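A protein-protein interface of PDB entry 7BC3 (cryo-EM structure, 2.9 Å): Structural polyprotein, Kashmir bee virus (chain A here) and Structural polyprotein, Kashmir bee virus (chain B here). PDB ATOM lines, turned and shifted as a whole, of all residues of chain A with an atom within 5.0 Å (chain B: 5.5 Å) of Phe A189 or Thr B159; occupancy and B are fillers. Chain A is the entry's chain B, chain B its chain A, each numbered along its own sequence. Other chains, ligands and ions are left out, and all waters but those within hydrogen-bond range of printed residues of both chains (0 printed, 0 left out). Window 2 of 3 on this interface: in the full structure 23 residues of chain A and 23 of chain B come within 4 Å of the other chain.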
ATOM      1  N   TYR A 146     -19.361  -8.849  18.795  1.00  0.00           N
ATOM      2  CA  TYR A 146     -18.868 -10.218  18.923  1.00  0.00           C
ATOM      3  C   TYR A 146     -17.363 -10.303  18.699  1.00  0.00           C
ATOM      4  O   TYR A 146     -16.848 -11.324  18.242  1.00  0.00           O
ATOM      5  CB  TYR A 146     -19.606 -11.154  17.964  1.00  0.00           C
ATOM      6  CG  TYR A 146     -21.103 -11.142  18.150  1.00  0.00           C
ATOM      7  CD1 TYR A 146     -21.724 -12.050  18.992  1.00  0.00           C
ATOM      8  CD2 TYR A 146     -21.896 -10.216  17.490  1.00  0.00           C
ATOM      9  CE1 TYR A 146     -23.089 -12.040  19.168  1.00  0.00           C
ATOM     10  CE2 TYR A 146     -23.261 -10.198  17.661  1.00  0.00           C
ATOM     11  CZ  TYR A 146     -23.853 -11.111  18.501  1.00  0.00           C
ATOM     12  OH  TYR A 146     -25.216 -11.097  18.675  1.00  0.00           O
ATOM     13  N   ALA A 187     -27.549  -5.606  20.134  1.00  0.00           N
ATOM     14  CA  ALA A 187     -26.569  -6.381  19.390  1.00  0.00           C
ATOM     15  C   ALA A 187     -26.756  -7.887  19.484  1.00  0.00           C
ATOM     16  O   ALA A 187     -26.038  -8.621  18.798  1.00  0.00           O
ATOM     17  CB  ALA A 187     -25.155  -6.033  19.874  1.00  0.00           C
ATOM     18  N   SER A 188     -27.682  -8.369  20.303  1.00  0.00           N
ATOM     19  CA  SER A 188     -27.878  -9.803  20.441  1.00  0.00           C
ATOM     20  C   SER A 188     -28.662 -10.357  19.262  1.00  0.00           C
ATOM     21  O   SER A 188     -29.638  -9.755  18.803  1.00  0.00           O
ATOM     22  CB  SER A 188     -28.612 -10.123  21.742  1.00  0.00           C
ATOM     23  OG  SER A 188     -28.775 -11.520  21.902  1.00  0.00           O
ATOM     24  N   PHE A 189     -28.219 -11.512  18.767  1.00  0.00           N
ATOM     25  CA  PHE A 189     -29.005 -12.266  17.802  1.00  0.00           C
ATOM     26  C   PHE A 189     -30.285 -12.808  18.418  1.00  0.00           C
ATOM     27  O   PHE A 189     -31.201 -13.193  17.685  1.00  0.00           O
ATOM     28  CB  PHE A 189     -28.175 -13.417  17.233  1.00  0.00           C
ATOM     29  CG  PHE A 189     -27.722 -14.405  18.267  1.00  0.00           C
ATOM     30  CD1 PHE A 189     -26.617 -14.147  19.056  1.00  0.00           C
ATOM     31  CD2 PHE A 189     -28.398 -15.597  18.446  1.00  0.00           C
ATOM     32  CE1 PHE A 189     -26.201 -15.049  20.004  1.00  0.00           C
ATOM     33  CE2 PHE A 189     -27.983 -16.504  19.394  1.00  0.00           C
ATOM     34  CZ  PHE A 189     -26.884 -16.230  20.174  1.00  0.00           C
ATOM     35  N   GLN A 190     -30.364 -12.844  19.745  1.00  0.00           N
ATOM     36  CA  GLN A 190     -31.551 -13.302  20.442  1.00  0.00           C
ATOM     37  C   GLN A 190     -32.621 -12.215  20.416  1.00  0.00           C
ATOM     38  O   GLN A 190     -32.419 -11.114  19.899  1.00  0.00           O
ATOM     39  CB  GLN A 190     -31.198 -13.691  21.875  1.00  0.00           C
ATOM     40  CG  GLN A 190     -30.013 -14.633  21.993  1.00  0.00           C
ATOM     41  CD  GLN A 190     -29.542 -14.812  23.420  1.00  0.00           C
ATOM     42  OE1 GLN A 190     -29.477 -15.929  23.928  1.00  0.00           O
ATOM     43  NE2 GLN A 190     -29.203 -13.707  24.073  1.00  0.00           N
ATOM     44  N   GLU A 191     -33.784 -12.527  20.986  1.00  0.00           N
ATOM     45  CA  GLU A 191     -34.867 -11.558  21.067  1.00  0.00           C
ATOM     46  C   GLU A 191     -34.694 -10.571  22.213  1.00  0.00           C
ATOM     47  O   GLU A 191     -35.419  -9.573  22.261  1.00  0.00           O
ATOM     48  CB  GLU A 191     -36.206 -12.280  21.214  1.00  0.00           C
ATOM     49  CG  GLU A 191     -36.446 -13.360  20.176  1.00  0.00           C
ATOM     50  CD  GLU A 191     -36.234 -12.868  18.760  1.00  0.00           C
ATOM     51  OE1 GLU A 191     -36.864 -11.860  18.381  1.00  0.00           O
ATOM     52  OE2 GLU A 191     -35.438 -13.491  18.026  1.00  0.00           O
ATOM     53  N   PHE A 202     -21.965  -8.718  23.832  1.00  0.00           N
ATOM     54  CA  PHE A 202     -22.188  -8.873  22.405  1.00  0.00           C
ATOM     55  C   PHE A 202     -21.512  -7.801  21.569  1.00  0.00           C
ATOM     56  O   PHE A 202     -21.542  -7.891  20.336  1.00  0.00           O
ATOM     57  CB  PHE A 202     -23.691  -8.869  22.111  1.00  0.00           C
ATOM     58  CG  PHE A 202     -24.443  -9.955  22.815  1.00  0.00           C
ATOM     59  CD1 PHE A 202     -24.556 -11.212  22.252  1.00  0.00           C
ATOM     60  CD2 PHE A 202     -25.030  -9.722  24.043  1.00  0.00           C
ATOM     61  CE1 PHE A 202     -25.243 -12.213  22.898  1.00  0.00           C
ATOM     62  CE2 PHE A 202     -25.719 -10.720  24.693  1.00  0.00           C
ATOM     63  CZ  PHE A 202     -25.825 -11.967  24.120  1.00  0.00           C
ATOM     64  N   PHE B  87     -23.484 -10.556  10.915  1.00  0.00           N
ATOM     65  CA  PHE B  87     -24.699 -11.352  10.940  1.00  0.00           C
ATOM     66  C   PHE B  87     -24.965 -11.964   9.575  1.00  0.00           C
ATOM     67  O   PHE B  87     -24.381 -11.578   8.561  1.00  0.00           O
ATOM     68  CB  PHE B  87     -25.919 -10.510  11.332  1.00  0.00           C
ATOM     69  CG  PHE B  87     -26.040 -10.220  12.798  1.00  0.00           C
ATOM     70  CD1 PHE B  87     -25.303 -10.908  13.743  1.00  0.00           C
ATOM     71  CD2 PHE B  87     -26.939  -9.267  13.230  1.00  0.00           C
ATOM     72  CE1 PHE B  87     -25.451 -10.633  15.081  1.00  0.00           C
ATOM     73  CE2 PHE B  87     -27.083  -8.986  14.564  1.00  0.00           C
ATOM     74  CZ  PHE B  87     -26.346  -9.679  15.492  1.00  0.00           C
ATOM     75  N   TYR B 151     -33.665 -18.301  15.925  1.00  0.00           N
ATOM     76  CA  TYR B 151     -33.320 -16.891  15.948  1.00  0.00           C
ATOM     77  C   TYR B 151     -33.561 -16.290  14.573  1.00  0.00           C
ATOM     78  O   TYR B 151     -33.443 -16.971  13.551  1.00  0.00           O
ATOM     79  CB  TYR B 151     -31.862 -16.693  16.358  1.00  0.00           C
ATOM     80  CG  TYR B 151     -31.521 -17.314  17.690  1.00  0.00           C
ATOM     81  CD1 TYR B 151     -31.923 -16.719  18.874  1.00  0.00           C
ATOM     82  CD2 TYR B 151     -30.803 -18.497  17.765  1.00  0.00           C
ATOM     83  CE1 TYR B 151     -31.618 -17.280  20.092  1.00  0.00           C
ATOM     84  CE2 TYR B 151     -30.494 -19.066  18.980  1.00  0.00           C
ATOM     85  CZ  TYR B 151     -30.903 -18.454  20.140  1.00  0.00           C
ATOM     86  OH  TYR B 151     -30.598 -19.017  21.355  1.00  0.00           O
ATOM     87  N   ARG B 152     -33.892 -15.000  14.558  1.00  0.00           N
ATOM     88  CA  ARG B 152     -34.169 -14.317  13.301  1.00  0.00           C
ATOM     89  C   ARG B 152     -32.895 -14.026  12.527  1.00  0.00           C
ATOM     90  O   ARG B 152     -32.936 -13.866  11.303  1.00  0.00           O
ATOM     91  CB  ARG B 152     -34.925 -13.019  13.570  1.00  0.00           C
ATOM     92  CG  ARG B 152     -34.120 -11.984  14.323  1.00  0.00           C
ATOM     93  CD  ARG B 152     -34.959 -10.769  14.645  1.00  0.00           C
ATOM     94  NE  ARG B 152     -35.992 -11.069  15.628  1.00  0.00           N
ATOM     95  CZ  ARG B 152     -37.009 -10.263  15.909  1.00  0.00           C
ATOM     96  NH1 ARG B 152     -37.136  -9.102  15.283  1.00  0.00           N
ATOM     97  NH2 ARG B 152     -37.903 -10.616  16.819  1.00  0.00           N
ATOM     98  N   LYS B 153     -31.769 -13.949  13.225  1.00  0.00           N
ATOM     99  CA  LYS B 153     -30.468 -13.723  12.625  1.00  0.00           C
ATOM    100  C   LYS B 153     -29.473 -14.688  13.251  1.00  0.00           C
ATOM    101  O   LYS B 153     -29.663 -15.151  14.376  1.00  0.00           O
ATOM    102  CB  LYS B 153     -29.997 -12.300  12.850  1.00  0.00           C
ATOM    103  CG  LYS B 153     -29.823 -11.992  14.313  1.00  0.00           C
ATOM    104  CD  LYS B 153     -29.746 -10.522  14.558  1.00  0.00           C
ATOM    105  CE  LYS B 153     -31.064  -9.911  14.889  1.00  0.00           C
ATOM    106  NZ  LYS B 153     -30.838  -8.480  15.193  1.00  0.00           N
ATOM    107  N   ILE B 154     -28.408 -14.974  12.512  1.00  0.00           N
ATOM    108  CA  ILE B 154     -27.344 -15.870  12.978  1.00  0.00           C
ATOM    109  C   ILE B 154     -26.050 -15.103  12.914  1.00  0.00           C
ATOM    110  O   ILE B 154     -25.721 -14.493  11.909  1.00  0.00           O
ATOM    111  CB  ILE B 154     -27.249 -17.149  12.102  1.00  0.00           C
ATOM    112  CG1 ILE B 154     -28.593 -17.871  12.071  1.00  0.00           C
ATOM    113  CG2 ILE B 154     -26.170 -18.054  12.646  1.00  0.00           C
ATOM    114  CD1 ILE B 154     -29.121 -18.257  13.428  1.00  0.00           C
ATOM    115  N   PRO B 155     -25.253 -15.097  14.001  1.00  0.00           N
ATOM    116  CA  PRO B 155     -23.952 -14.435  13.954  1.00  0.00           C
ATOM    117  C   PRO B 155     -22.892 -15.345  13.352  1.00  0.00           C
ATOM    118  O   PRO B 155     -23.060 -16.557  13.221  1.00  0.00           O
ATOM    119  CB  PRO B 155     -23.659 -14.138  15.426  1.00  0.00           C
ATOM    120  CG  PRO B 155     -24.359 -15.201  16.161  1.00  0.00           C
ATOM    121  CD  PRO B 155     -25.565 -15.591  15.350  1.00  0.00           C
ATOM    122  N   ALA B 157     -19.973 -15.759  14.723  1.00  0.00           N
ATOM    123  CA  ALA B 157     -19.091 -16.007  15.850  1.00  0.00           C
ATOM    124  C   ALA B 157     -19.562 -17.252  16.594  1.00  0.00           C
ATOM    125  O   ALA B 157     -20.555 -17.882  16.228  1.00  0.00           O
ATOM    126  CB  ALA B 157     -19.061 -14.795  16.785  1.00  0.00           C
ATOM    127  N   SER B 158     -18.831 -17.602  17.646  1.00  0.00           N
ATOM    128  CA  SER B 158     -19.189 -18.747  18.464  1.00  0.00           C
ATOM    129  C   SER B 158     -20.287 -18.376  19.451  1.00  0.00           C
ATOM    130  O   SER B 158     -20.343 -17.255  19.967  1.00  0.00           O
ATOM    131  CB  SER B 158     -17.972 -19.271  19.219  1.00  0.00           C
ATOM    132  OG  SER B 158     -17.395 -18.254  20.016  1.00  0.00           O
ATOM    133  N   THR B 159     -21.169 -19.339  19.709  1.00  0.00           N
ATOM    134  CA  THR B 159     -22.300 -19.146  20.601  1.00  0.00           C
ATOM    135  C   THR B 159     -22.278 -20.204  21.695  1.00  0.00           C
ATOM    136  O   THR B 159     -21.593 -21.226  21.596  1.00  0.00           O
ATOM    137  CB  THR B 159     -23.638 -19.222  19.853  1.00  0.00           C
ATOM    138  OG1 THR B 159     -23.679 -20.417  19.067  1.00  0.00           O
ATOM    139  CG2 THR B 159     -23.827 -18.015  18.956  1.00  0.00           C
ATOM    140  N   THR B 160     -23.042 -19.934  22.757  1.00  0.00           N
ATOM    141  CA  THR B 160     -23.253 -20.938  23.795  1.00  0.00           C
ATOM    142  C   THR B 160     -24.265 -21.991  23.365  1.00  0.00           C
ATOM    143  O   THR B 160     -24.140 -23.163  23.743  1.00  0.00           O
ATOM    144  CB  THR B 160     -23.732 -20.270  25.087  1.00  0.00           C
ATOM    145  OG1 THR B 160     -23.044 -19.033  25.282  1.00  0.00           O
ATOM    146  CG2 THR B 160     -23.597 -21.129  26.325  1.00  0.00           C
ATOM    147  N   ASP B 161     -25.256 -21.599  22.570  1.00  0.00           N
ATOM    148  CA  ASP B 161     -26.269 -22.530  22.110  1.00  0.00           C
ATOM    149  C   ASP B 161     -25.757 -23.314  20.908  1.00  0.00           C
ATOM    150  O   ASP B 161     -24.797 -22.923  20.236  1.00  0.00           O
ATOM    151  CB  ASP B 161     -27.555 -21.785  21.752  1.00  0.00           C
ATOM    152  CG  ASP B 161     -28.756 -22.700  21.673  1.00  0.00           C
ATOM    153  OD1 ASP B 161     -28.573 -23.932  21.792  1.00  0.00           O
ATOM    154  OD2 ASP B 161     -29.887 -22.198  21.492  1.00  0.00           O
ATOM    155  N   LYS B 162     -26.412 -24.439  20.651  1.00  0.00           N
ATOM    156  CA  LYS B 162     -26.031 -25.319  19.560  1.00  0.00           C
ATOM    157  C   LYS B 162     -27.285 -25.977  19.009  1.00  0.00           C
ATOM    158  O   LYS B 162     -28.181 -26.355  19.768  1.00  0.00           O
ATOM    159  CB  LYS B 162     -25.031 -26.382  20.024  1.00  0.00           C
ATOM    160  CG  LYS B 162     -24.037 -26.790  18.958  1.00  0.00           C
ATOM    161  CD  LYS B 162     -23.035 -27.796  19.491  1.00  0.00           C
ATOM    162  CE  LYS B 162     -23.702 -29.110  19.837  1.00  0.00           C
ATOM    163  NZ  LYS B 162     -22.708 -30.175  20.121  1.00  0.00           N
ATOM    164  N   TYR B 164     -29.283 -24.335  16.831  1.00  0.00           N
ATOM    165  CA  TYR B 164     -30.262 -23.268  16.695  1.00  0.00           C
ATOM    166  C   TYR B 164     -30.572 -22.938  15.243  1.00  0.00           C
ATOM    167  O   TYR B 164     -31.411 -22.070  14.984  1.00  0.00           O
ATOM    168  CB  TYR B 164     -29.781 -22.004  17.418  1.00  0.00           C
ATOM    169  CG  TYR B 164     -28.365 -21.583  17.091  1.00  0.00           C
ATOM    170  CD1 TYR B 164     -27.291 -22.070  17.819  1.00  0.00           C
ATOM    171  CD2 TYR B 164     -28.105 -20.688  16.065  1.00  0.00           C
ATOM    172  CE1 TYR B 164     -25.999 -21.689  17.530  1.00  0.00           C
ATOM    173  CE2 TYR B 164     -26.816 -20.299  15.768  1.00  0.00           C
ATOM    174  CZ  TYR B 164     -25.767 -20.802  16.503  1.00  0.00           C
ATOM    175  OH  TYR B 164     -24.478 -20.417  16.212  1.00  0.00           O
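Of the 7 printed residues of chain A, 5 touch a printed residue of chain B.
Hydrophobic or aromatic side chains of chain A that line the printed part of chain B: Tyr A146 and Phe A189.
Along chain A the printed residues that touch a printed residue of chain B span positions 146 to 191.
Of the 13 printed residues of chain B, 7 touch a printed residue of chain A.
Hydrophobic or aromatic side chains of chain B that line the printed part of chain A: Phe B87, Tyr B151, Pro B155 and Ala B157.
Along chain B the printed residues that touch a printed residue of chain A span positions 87 to 159.
Among the printed residues, 9 pairs touch across the chains.
OH of Tyr B151 lies within hydrogen-bond range of OD2 of Asp B161 (3.3 Å).
OG1 of Thr B159 sits at hydrogen-bond distance from O of Asp B161 (3.0 Å).
OG1 of Thr B159 lies within hydrogen-bond range of OH of Tyr B164 (3.0 Å).
The side-chain hydroxyl (OH) of Tyr A146 lies within hydrogen-bond range of the backbone carbonyl oxygen (O) of Ala A187 (2.6 Å).
The side-chain hydroxyl of Tyr A146 sits at hydrogen-bond distance from the backbone NH of Phe A189.
O of Phe A202 lies within hydrogen-bond range of N of Tyr A146 (2.8 Å).
NE of Arg B152 lies within salt-bridge range of OE1 of Glu A191 (3.0 Å).
Of chain B, only Tyr B151 (3.6 Å), Lys B153 (3.6 Å), Pro B155 (3.8 Å) and Thr B159 (3.7 Å) come within 4 Å of Phe A189.
Printed residues of chain B within 4 Å of Gln A190: Tyr B151 (3.6 Å).
Of the printed residues of chain B, Glu A191 touches Arg B152 (2.3 Å).
Of chain A, only Phe A189 (3.7 Å) comes within 4 Å of Thr B159.
The nearest printed residue of chain B that does not touch Ala A187 is Lys B153 (5.9 Å).
Among the printed residues, pairs that only touch across the chains: Tyr A146 with Phe B87 (3.4 Å), Tyr A146 with Ala B157 (3.9 Å), Ala A187 with Phe B87 (3.5 Å), Phe A189 with Tyr B151 (3.6 Å), Phe A189 with Lys B153 (3.6 Å), Phe A189 with Pro B155 (3.8 Å), Phe A189 with Thr B159 (3.7 Å) and Gln A190 with Tyr B151 (3.6 Å).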
